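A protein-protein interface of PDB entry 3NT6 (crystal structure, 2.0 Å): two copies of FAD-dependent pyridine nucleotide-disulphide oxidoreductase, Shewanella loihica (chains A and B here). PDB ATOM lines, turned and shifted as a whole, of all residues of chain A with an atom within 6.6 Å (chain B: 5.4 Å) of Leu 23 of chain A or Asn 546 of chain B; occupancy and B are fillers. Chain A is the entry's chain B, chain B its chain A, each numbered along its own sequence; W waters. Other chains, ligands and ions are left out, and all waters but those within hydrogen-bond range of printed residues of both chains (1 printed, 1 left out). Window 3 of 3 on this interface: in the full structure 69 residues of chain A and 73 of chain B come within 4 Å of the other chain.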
ATOM      1  N   ALA A  18      -5.253 -16.923   6.203  1.00  0.00           N
ATOM      2  CA  ALA A  18      -6.614 -16.442   6.236  1.00  0.00           C
ATOM      3  C   ALA A  18      -7.440 -17.353   5.346  1.00  0.00           C
ATOM      4  O   ALA A  18      -8.529 -17.739   5.769  1.00  0.00           O
ATOM      5  CB  ALA A  18      -6.769 -14.995   5.890  1.00  0.00           C
ATOM      6  N   ARG A  19      -6.940 -17.706   4.169  1.00  0.00           N
ATOM      7  CA  ARG A  19      -7.598 -18.648   3.266  1.00  0.00           C
ATOM      8  C   ARG A  19      -7.852 -20.035   3.949  1.00  0.00           C
ATOM      9  O   ARG A  19      -8.897 -20.701   3.734  1.00  0.00           O
ATOM     10  CB  ARG A  19      -6.798 -18.801   1.970  1.00  0.00           C
ATOM     11  CG  ARG A  19      -7.379 -19.884   0.938  1.00  0.00           C
ATOM     12  CD  ARG A  19      -8.733 -19.409   0.350  1.00  0.00           C
ATOM     13  NE  ARG A  19      -9.198 -20.420  -0.617  1.00  0.00           N
ATOM     14  CZ  ARG A  19     -10.418 -20.531  -1.172  1.00  0.00           C
ATOM     15  NH1 ARG A  19     -11.449 -19.741  -0.868  1.00  0.00           N
ATOM     16  NH2 ARG A  19     -10.573 -21.443  -2.102  1.00  0.00           N
ATOM     17  N   ALA A  20      -6.870 -20.452   4.742  1.00  0.00           N
ATOM     18  CA  ALA A  20      -6.786 -21.778   5.272  1.00  0.00           C
ATOM     19  C   ALA A  20      -7.938 -21.814   6.316  1.00  0.00           C
ATOM     20  O   ALA A  20      -8.682 -22.777   6.370  1.00  0.00           O
ATOM     21  CB  ALA A  20      -5.387 -22.003   5.904  1.00  0.00           C
ATOM     22  N   ARG A  21      -8.131 -20.706   7.031  1.00  0.00           N
ATOM     23  CA  ARG A  21      -9.214 -20.619   8.009  1.00  0.00           C
ATOM     24  C   ARG A  21     -10.597 -20.632   7.291  1.00  0.00           C
ATOM     25  O   ARG A  21     -11.545 -21.299   7.780  1.00  0.00           O
ATOM     26  CB  ARG A  21      -9.058 -19.445   8.938  1.00  0.00           C
ATOM     27  CG  ARG A  21     -10.301 -19.355  10.069  1.00  0.00           C
ATOM     28  CD  ARG A  21     -10.327 -20.702  10.828  1.00  0.00           C
ATOM     29  NE  ARG A  21      -9.236 -20.897  11.819  1.00  0.00           N
ATOM     30  CZ  ARG A  21      -8.675 -22.066  12.168  1.00  0.00           C
ATOM     31  NH1 ARG A  21      -9.071 -23.266  11.636  1.00  0.00           N
ATOM     32  NH2 ARG A  21      -7.688 -22.063  13.094  1.00  0.00           N
ATOM     33  N   ARG A  22     -10.694 -19.946   6.151  1.00  0.00           N
ATOM     34  CA  ARG A  22     -11.997 -19.945   5.388  1.00  0.00           C
ATOM     35  C   ARG A  22     -12.239 -21.409   4.895  1.00  0.00           C
ATOM     36  O   ARG A  22     -13.394 -21.875   4.825  1.00  0.00           O
ATOM     37  CB  ARG A  22     -12.032 -18.891   4.290  1.00  0.00           C
ATOM     38  CG  ARG A  22     -11.921 -17.408   4.963  1.00  0.00           C
ATOM     39  CD  ARG A  22     -12.139 -16.433   3.869  1.00  0.00           C
ATOM     40  NE  ARG A  22     -11.071 -16.359   2.903  1.00  0.00           N
ATOM     41  CZ  ARG A  22     -10.007 -15.569   2.999  1.00  0.00           C
ATOM     42  NH1 ARG A  22      -9.758 -14.819   4.123  1.00  0.00           N
ATOM     43  NH2 ARG A  22      -9.210 -15.588   1.957  1.00  0.00           N
ATOM     44  N   LEU A  23     -11.164 -22.162   4.670  1.00  0.00           N
ATOM     45  CA  LEU A  23     -11.316 -23.547   4.241  1.00  0.00           C
ATOM     46  C   LEU A  23     -11.722 -24.535   5.320  1.00  0.00           C
ATOM     47  O   LEU A  23     -12.289 -25.578   4.989  1.00  0.00           O
ATOM     48  CB  LEU A  23     -10.071 -24.081   3.470  1.00  0.00           C
ATOM     49  CG  LEU A  23      -9.849 -23.434   2.144  1.00  0.00           C
ATOM     50  CD1 LEU A  23      -8.411 -23.748   1.724  1.00  0.00           C
ATOM     51  CD2 LEU A  23     -10.814 -23.910   1.105  1.00  0.00           C
ATOM     52  N   SER A  24     -11.411 -24.247   6.577  1.00  0.00           N
ATOM     53  CA  SER A  24     -11.628 -25.232   7.706  1.00  0.00           C
ATOM     54  C   SER A  24     -11.615 -24.568   9.093  1.00  0.00           C
ATOM     55  O   SER A  24     -10.664 -23.818   9.471  1.00  0.00           O
ATOM     56  CB  SER A  24     -10.593 -26.364   7.675  1.00  0.00           C
ATOM     57  OG  SER A  24     -10.467 -26.957   8.977  1.00  0.00           O
ATOM     58  N   GLU A  25     -12.684 -24.790   9.866  1.00  0.00           N
ATOM     59  CA  GLU A  25     -12.732 -24.338  11.293  1.00  0.00           C
ATOM     60  C   GLU A  25     -11.987 -25.229  12.334  1.00  0.00           C
ATOM     61  O   GLU A  25     -11.730 -24.813  13.488  1.00  0.00           O
ATOM     62  CB  GLU A  25     -14.215 -24.146  11.733  1.00  0.00           C
ATOM     63  CG  GLU A  25     -14.894 -22.745  11.384  1.00  0.00           C
ATOM     64  CD  GLU A  25     -14.195 -21.482  11.994  1.00  0.00           C
ATOM     65  OE1 GLU A  25     -13.820 -21.422  13.241  1.00  0.00           O
ATOM     66  OE2 GLU A  25     -14.073 -20.496  11.214  1.00  0.00           O
ATOM     67  N   THR A  26     -11.588 -26.419  11.908  1.00  0.00           N
ATOM     68  CA  THR A  26     -11.005 -27.455  12.775  1.00  0.00           C
ATOM     69  C   THR A  26      -9.481 -27.454  12.694  1.00  0.00           C
ATOM     70  O   THR A  26      -8.779 -27.796  13.677  1.00  0.00           O
ATOM     71  CB  THR A  26     -11.566 -28.873  12.424  1.00  0.00           C
ATOM     72  OG1 THR A  26     -11.222 -29.204  11.079  1.00  0.00           O
ATOM     73  CG2 THR A  26     -13.071 -28.850  12.541  1.00  0.00           C
ATOM     74  N   ARG A 329      -2.637 -17.981  -1.033  1.00  0.00           N
ATOM     75  CA  ARG A 329      -4.001 -18.472  -0.999  1.00  0.00           C
ATOM     76  C   ARG A 329      -4.079 -19.864  -1.661  1.00  0.00           C
ATOM     77  O   ARG A 329      -4.694 -20.775  -1.122  1.00  0.00           O
ATOM     78  CB  ARG A 329      -4.896 -17.427  -1.761  1.00  0.00           C
ATOM     79  CG  ARG A 329      -6.351 -17.787  -1.896  1.00  0.00           C
ATOM     80  CD  ARG A 329      -7.035 -16.748  -2.976  1.00  0.00           C
ATOM     81  NE  ARG A 329      -8.485 -17.023  -3.079  1.00  0.00           N
ATOM     82  CZ  ARG A 329      -9.036 -17.935  -3.879  1.00  0.00           C
ATOM     83  NH1 ARG A 329      -8.277 -18.648  -4.714  1.00  0.00           N
ATOM     84  NH2 ARG A 329     -10.368 -18.144  -3.860  1.00  0.00           N
ATOM     85  N   ALA A 332      -2.726 -22.626   0.363  1.00  0.00           N
ATOM     86  CA  ALA A 332      -3.637 -23.127   1.491  1.00  0.00           C
ATOM     87  C   ALA A 332      -4.644 -24.052   0.805  1.00  0.00           C
ATOM     88  O   ALA A 332      -5.042 -25.006   1.390  1.00  0.00           O
ATOM     89  CB  ALA A 332      -4.389 -21.984   2.067  1.00  0.00           C
ATOM     90  N   ASP A 333      -5.052 -23.749  -0.451  1.00  0.00           N
ATOM     91  CA  ASP A 333      -6.047 -24.700  -1.111  1.00  0.00           C
ATOM     92  C   ASP A 333      -5.446 -26.090  -1.241  1.00  0.00           C
ATOM     93  O   ASP A 333      -6.122 -27.091  -1.030  1.00  0.00           O
ATOM     94  CB  ASP A 333      -6.403 -24.174  -2.504  1.00  0.00           C
ATOM     95  CG  ASP A 333      -7.349 -22.973  -2.456  1.00  0.00           C
ATOM     96  OD1 ASP A 333      -7.784 -22.595  -1.326  1.00  0.00           O
ATOM     97  OD2 ASP A 333      -7.588 -22.386  -3.556  1.00  0.00           O
ATOM     98  N   ASN A 334      -4.190 -26.121  -1.684  1.00  0.00           N
ATOM     99  CA  ASN A 334      -3.383 -27.386  -1.835  1.00  0.00           C
ATOM    100  C   ASN A 334      -3.143 -28.168  -0.601  1.00  0.00           C
ATOM    101  O   ASN A 334      -3.272 -29.412  -0.580  1.00  0.00           O
ATOM    102  CB  ASN A 334      -2.154 -27.147  -2.778  1.00  0.00           C
ATOM    103  CG  ASN A 334      -2.616 -26.737  -4.174  1.00  0.00           C
ATOM    104  OD1 ASN A 334      -3.768 -27.007  -4.505  1.00  0.00           O
ATOM    105  ND2 ASN A 334      -1.783 -26.009  -4.956  1.00  0.00           N
ATOM    106  N   MET A 335      -2.936 -27.458   0.502  1.00  0.00           N
ATOM    107  CA  MET A 335      -2.928 -28.120   1.776  1.00  0.00           C
ATOM    108  C   MET A 335      -4.199 -28.766   2.138  1.00  0.00           C
ATOM    109  O   MET A 335      -4.186 -29.630   2.950  1.00  0.00           O
ATOM    110  CB  MET A 335      -2.609 -27.123   2.835  1.00  0.00           C
ATOM    111  CG  MET A 335      -1.206 -26.780   2.747  1.00  0.00           C
ATOM    112  SD  MET A 335      -0.889 -25.399   4.150  1.00  0.00           S
ATOM    113  CE  MET A 335       0.857 -24.950   3.550  1.00  0.00           C
ATOM    114  N   PHE A 336      -5.327 -28.361   1.564  1.00  0.00           N
ATOM    115  CA  PHE A 336      -6.517 -29.178   1.875  1.00  0.00           C
ATOM    116  C   PHE A 336      -6.909 -30.080   0.705  1.00  0.00           C
ATOM    117  O   PHE A 336      -8.021 -30.566   0.657  1.00  0.00           O
ATOM    118  CB  PHE A 336      -7.659 -28.257   2.253  1.00  0.00           C
ATOM    119  CG  PHE A 336      -7.468 -27.623   3.571  1.00  0.00           C
ATOM    120  CD1 PHE A 336      -7.931 -28.235   4.724  1.00  0.00           C
ATOM    121  CD2 PHE A 336      -6.829 -26.421   3.647  1.00  0.00           C
ATOM    122  CE1 PHE A 336      -7.722 -27.633   5.981  1.00  0.00           C
ATOM    123  CE2 PHE A 336      -6.622 -25.834   4.837  1.00  0.00           C
ATOM    124  CZ  PHE A 336      -7.061 -26.422   6.013  1.00  0.00           C
ATOM    125  N   ARG A 338      -6.869 -29.626  -2.752  1.00  0.00           N
ATOM    126  CA  ARG A 338      -7.559 -29.177  -3.923  1.00  0.00           C
ATOM    127  C   ARG A 338      -6.767 -29.223  -5.189  1.00  0.00           C
ATOM    128  O   ARG A 338      -7.311 -28.895  -6.241  1.00  0.00           O
ATOM    129  CB  ARG A 338      -8.027 -27.757  -3.753  1.00  0.00           C
ATOM    130  CG  ARG A 338      -9.076 -27.698  -2.713  1.00  0.00           C
ATOM    131  CD  ARG A 338      -9.866 -26.376  -2.841  1.00  0.00           C
ATOM    132  NE  ARG A 338     -10.997 -26.582  -1.932  1.00  0.00           N
ATOM    133  CZ  ARG A 338     -12.080 -25.844  -1.902  1.00  0.00           C
ATOM    134  NH1 ARG A 338     -12.193 -24.858  -2.756  1.00  0.00           N
ATOM    135  NH2 ARG A 338     -13.012 -26.122  -1.018  1.00  0.00           N
ATOM    136  N   TYR B 541     -19.806 -16.243   6.699  1.00  0.00           N
ATOM    137  CA  TYR B 541     -20.472 -17.282   6.034  1.00  0.00           C
ATOM    138  C   TYR B 541     -19.606 -18.540   6.145  1.00  0.00           C
ATOM    139  O   TYR B 541     -20.125 -19.653   6.397  1.00  0.00           O
ATOM    140  CB  TYR B 541     -20.620 -16.936   4.562  1.00  0.00           C
ATOM    141  CG  TYR B 541     -20.970 -18.081   3.703  1.00  0.00           C
ATOM    142  CD1 TYR B 541     -22.317 -18.434   3.483  1.00  0.00           C
ATOM    143  CD2 TYR B 541     -19.989 -18.824   3.049  1.00  0.00           C
ATOM    144  CE1 TYR B 541     -22.670 -19.559   2.673  1.00  0.00           C
ATOM    145  CE2 TYR B 541     -20.336 -19.956   2.231  1.00  0.00           C
ATOM    146  CZ  TYR B 541     -21.689 -20.280   2.050  1.00  0.00           C
ATOM    147  OH  TYR B 541     -22.040 -21.330   1.210  1.00  0.00           O
ATOM    148  N   ARG B 542     -18.310 -18.398   5.841  1.00  0.00           N
ATOM    149  CA  ARG B 542     -17.426 -19.501   5.948  1.00  0.00           C
ATOM    150  C   ARG B 542     -17.403 -20.104   7.345  1.00  0.00           C
ATOM    151  O   ARG B 542     -17.475 -21.320   7.505  1.00  0.00           O
ATOM    152  CB  ARG B 542     -16.012 -19.183   5.395  1.00  0.00           C
ATOM    153  CG  ARG B 542     -15.967 -19.000   3.833  1.00  0.00           C
ATOM    154  CD  ARG B 542     -16.447 -20.257   3.029  1.00  0.00           C
ATOM    155  NE  ARG B 542     -15.803 -21.510   3.454  1.00  0.00           N
ATOM    156  CZ  ARG B 542     -16.073 -22.681   2.875  1.00  0.00           C
ATOM    157  NH1 ARG B 542     -17.020 -22.735   1.922  1.00  0.00           N
ATOM    158  NH2 ARG B 542     -15.465 -23.792   3.268  1.00  0.00           N
ATOM    159  N   GLN B 543     -17.206 -19.294   8.361  1.00  0.00           N
ATOM    160  CA  GLN B 543     -17.343 -19.799   9.711  1.00  0.00           C
ATOM    161  C   GLN B 543     -18.635 -20.682   9.955  1.00  0.00           C
ATOM    162  O   GLN B 543     -18.580 -21.761  10.589  1.00  0.00           O
ATOM    163  CB  GLN B 543     -17.374 -18.608  10.707  1.00  0.00           C
ATOM    164  CG  GLN B 543     -16.049 -17.856  10.966  1.00  0.00           C
ATOM    165  CD  GLN B 543     -16.081 -16.923  12.211  1.00  0.00           C
ATOM    166  OE1 GLN B 543     -15.341 -15.876  12.328  1.00  0.00           O
ATOM    167  NE2 GLN B 543     -16.862 -17.354  13.205  1.00  0.00           N
ATOM    168  N   LEU B 544     -19.794 -20.204   9.502  1.00  0.00           N
ATOM    169  CA  LEU B 544     -21.034 -20.875   9.717  1.00  0.00           C
ATOM    170  C   LEU B 544     -21.102 -22.215   8.967  1.00  0.00           C
ATOM    171  O   LEU B 544     -21.266 -23.262   9.636  1.00  0.00           O
ATOM    172  CB  LEU B 544     -22.245 -19.917   9.521  1.00  0.00           C
ATOM    173  CG  LEU B 544     -22.369 -18.736  10.488  1.00  0.00           C
ATOM    174  CD1 LEU B 544     -23.528 -17.916  10.160  1.00  0.00           C
ATOM    175  CD2 LEU B 544     -22.496 -18.998  12.001  1.00  0.00           C
ATOM    176  N   VAL B 545     -20.880 -22.229   7.617  1.00  0.00           N
ATOM    177  CA  VAL B 545     -20.947 -23.478   6.853  1.00  0.00           C
ATOM    178  C   VAL B 545     -19.891 -24.459   7.304  1.00  0.00           C
ATOM    179  O   VAL B 545     -20.148 -25.682   7.222  1.00  0.00           O
ATOM    180  CB  VAL B 545     -20.864 -23.331   5.356  1.00  0.00           C
ATOM    181  CG1 VAL B 545     -22.079 -22.512   4.916  1.00  0.00           C
ATOM    182  CG2 VAL B 545     -19.619 -22.555   4.955  1.00  0.00           C
ATOM    183  N   ASN B 546     -18.731 -23.972   7.760  1.00  0.00           N
ATOM    184  CA  ASN B 546     -17.718 -24.904   8.283  1.00  0.00           C
ATOM    185  C   ASN B 546     -18.209 -25.592   9.533  1.00  0.00           C
ATOM    186  O   ASN B 546     -17.787 -26.680   9.856  1.00  0.00           O
ATOM    187  CB  ASN B 546     -16.402 -24.172   8.583  1.00  0.00           C
ATOM    188  CG  ASN B 546     -15.596 -23.922   7.324  1.00  0.00           C
ATOM    189  OD1 ASN B 546     -14.777 -22.968   7.238  1.00  0.00           O
ATOM    190  ND2 ASN B 546     -15.849 -24.731   6.313  1.00  0.00           N
ATOM    191  N   ASN B 547     -19.099 -24.948  10.261  1.00  0.00           N
ATOM    192  CA  ASN B 547     -19.703 -25.539  11.426  1.00  0.00           C
ATOM    193  C   ASN B 547     -21.075 -26.176  11.157  1.00  0.00           C
ATOM    194  O   ASN B 547     -21.807 -26.368  12.095  1.00  0.00           O
ATOM    195  CB  ASN B 547     -19.843 -24.502  12.531  1.00  0.00           C
ATOM    196  CG  ASN B 547     -18.517 -24.179  13.191  1.00  0.00           C
ATOM    197  OD1 ASN B 547     -17.882 -23.141  12.900  1.00  0.00           O
ATOM    198  ND2 ASN B 547     -18.071 -25.076  14.070  1.00  0.00           N
ATOM    199  N   GLY B 548     -21.460 -26.414   9.896  1.00  0.00           N
ATOM    200  CA  GLY B 548     -22.675 -27.185   9.623  1.00  0.00           C
ATOM    201  C   GLY B 548     -23.990 -26.397   9.497  1.00  0.00           C
ATOM    202  O   GLY B 548     -25.071 -27.015   9.322  1.00  0.00           O
HETATM  203  O   HOH W   1     -15.381 -22.719  14.688  1.00  0.00           O
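O of Arg 22 of chain A is in hydrogen-bond range of NE of Arg 542 of chain B, 2.8 Å away. OD1 of Asn 546 of chain B sits close to O of Arg 22 of chain A, 3.0 Å away.
The backbone carbonyl oxygen of Arg 542 of chain B sits close to the side-chain amide oxygen of Asn 546 of chain B, at 3.2 Å. The backbone carbonyl oxygen (O) of Gln 543 of chain B lies close to the side-chain amide oxygen (OD1) of Asn 547 of chain B. The guanidinium group of Arg 21 of chain A sits at hydrogen-bond distance from the backbone carbonyl oxygen of Ser 24 of chain A (2.7 Å). OG of Ser 24 of chain A sits at hydrogen-bond distance from OG1 of Thr 26 of chain A, at 3.2 Å.
Water W1 lies within hydrogen-bond range of OE1 of Glu 25 of chain A (2.5 Å) and OD1 of Asn 547 of chain B (3.1 Å).
Among the printed residues, 8 pairs touch across the chains. Among the printed residues, no Asp or Glu carboxylate lies within 4 Å of a Lys or Arg side-chain nitrogen of the other chain.
No position is printed for both chains.
Printed residues of chain B within 4 Å of Arg 21 of chain A: Asn 546. Leu 23 of chain A touches just one residue of chain B: Asn 546 (3.9 Å). Of the printed residues of chain B, Glu 25 of chain A touches Gln 543, Asn 546 and Asn 547. Asn 334 of chain A touches none of the printed residues of chain B. Printed residues of chain A within 4 Å of Arg 542 of chain B: Arg 22 (2.8 Å). Asn 546 of chain B touches just these residues of chain A: Arg 21 (3.7 Å), Arg 22 (3.0 Å), Leu 23 (3.9 Å), Ser 24 (3.7 Å) and Glu 25 (3.5 Å). Of the printed residues of chain A, Asn 547 of chain B touches Glu 25.
O of Arg 21 of chain A touches OD1 of Asn 546 of chain B (3.7 Å). O of Leu 23 of chain A touches ND2 of Asn 546 of chain B, at 3.9 Å. Ser 24 of chain A touches Asn 546 of chain B (N to OD1, 3.7 Å). OE2 of Glu 25 of chain A touches CG of Gln 543 of chain B (3.3 Å). Glu 25 of chain A touches Asn 546 of chain B. Glu 25 of chain A touches Asn 547 of chain B (CG to OD1, 3.4 Å).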
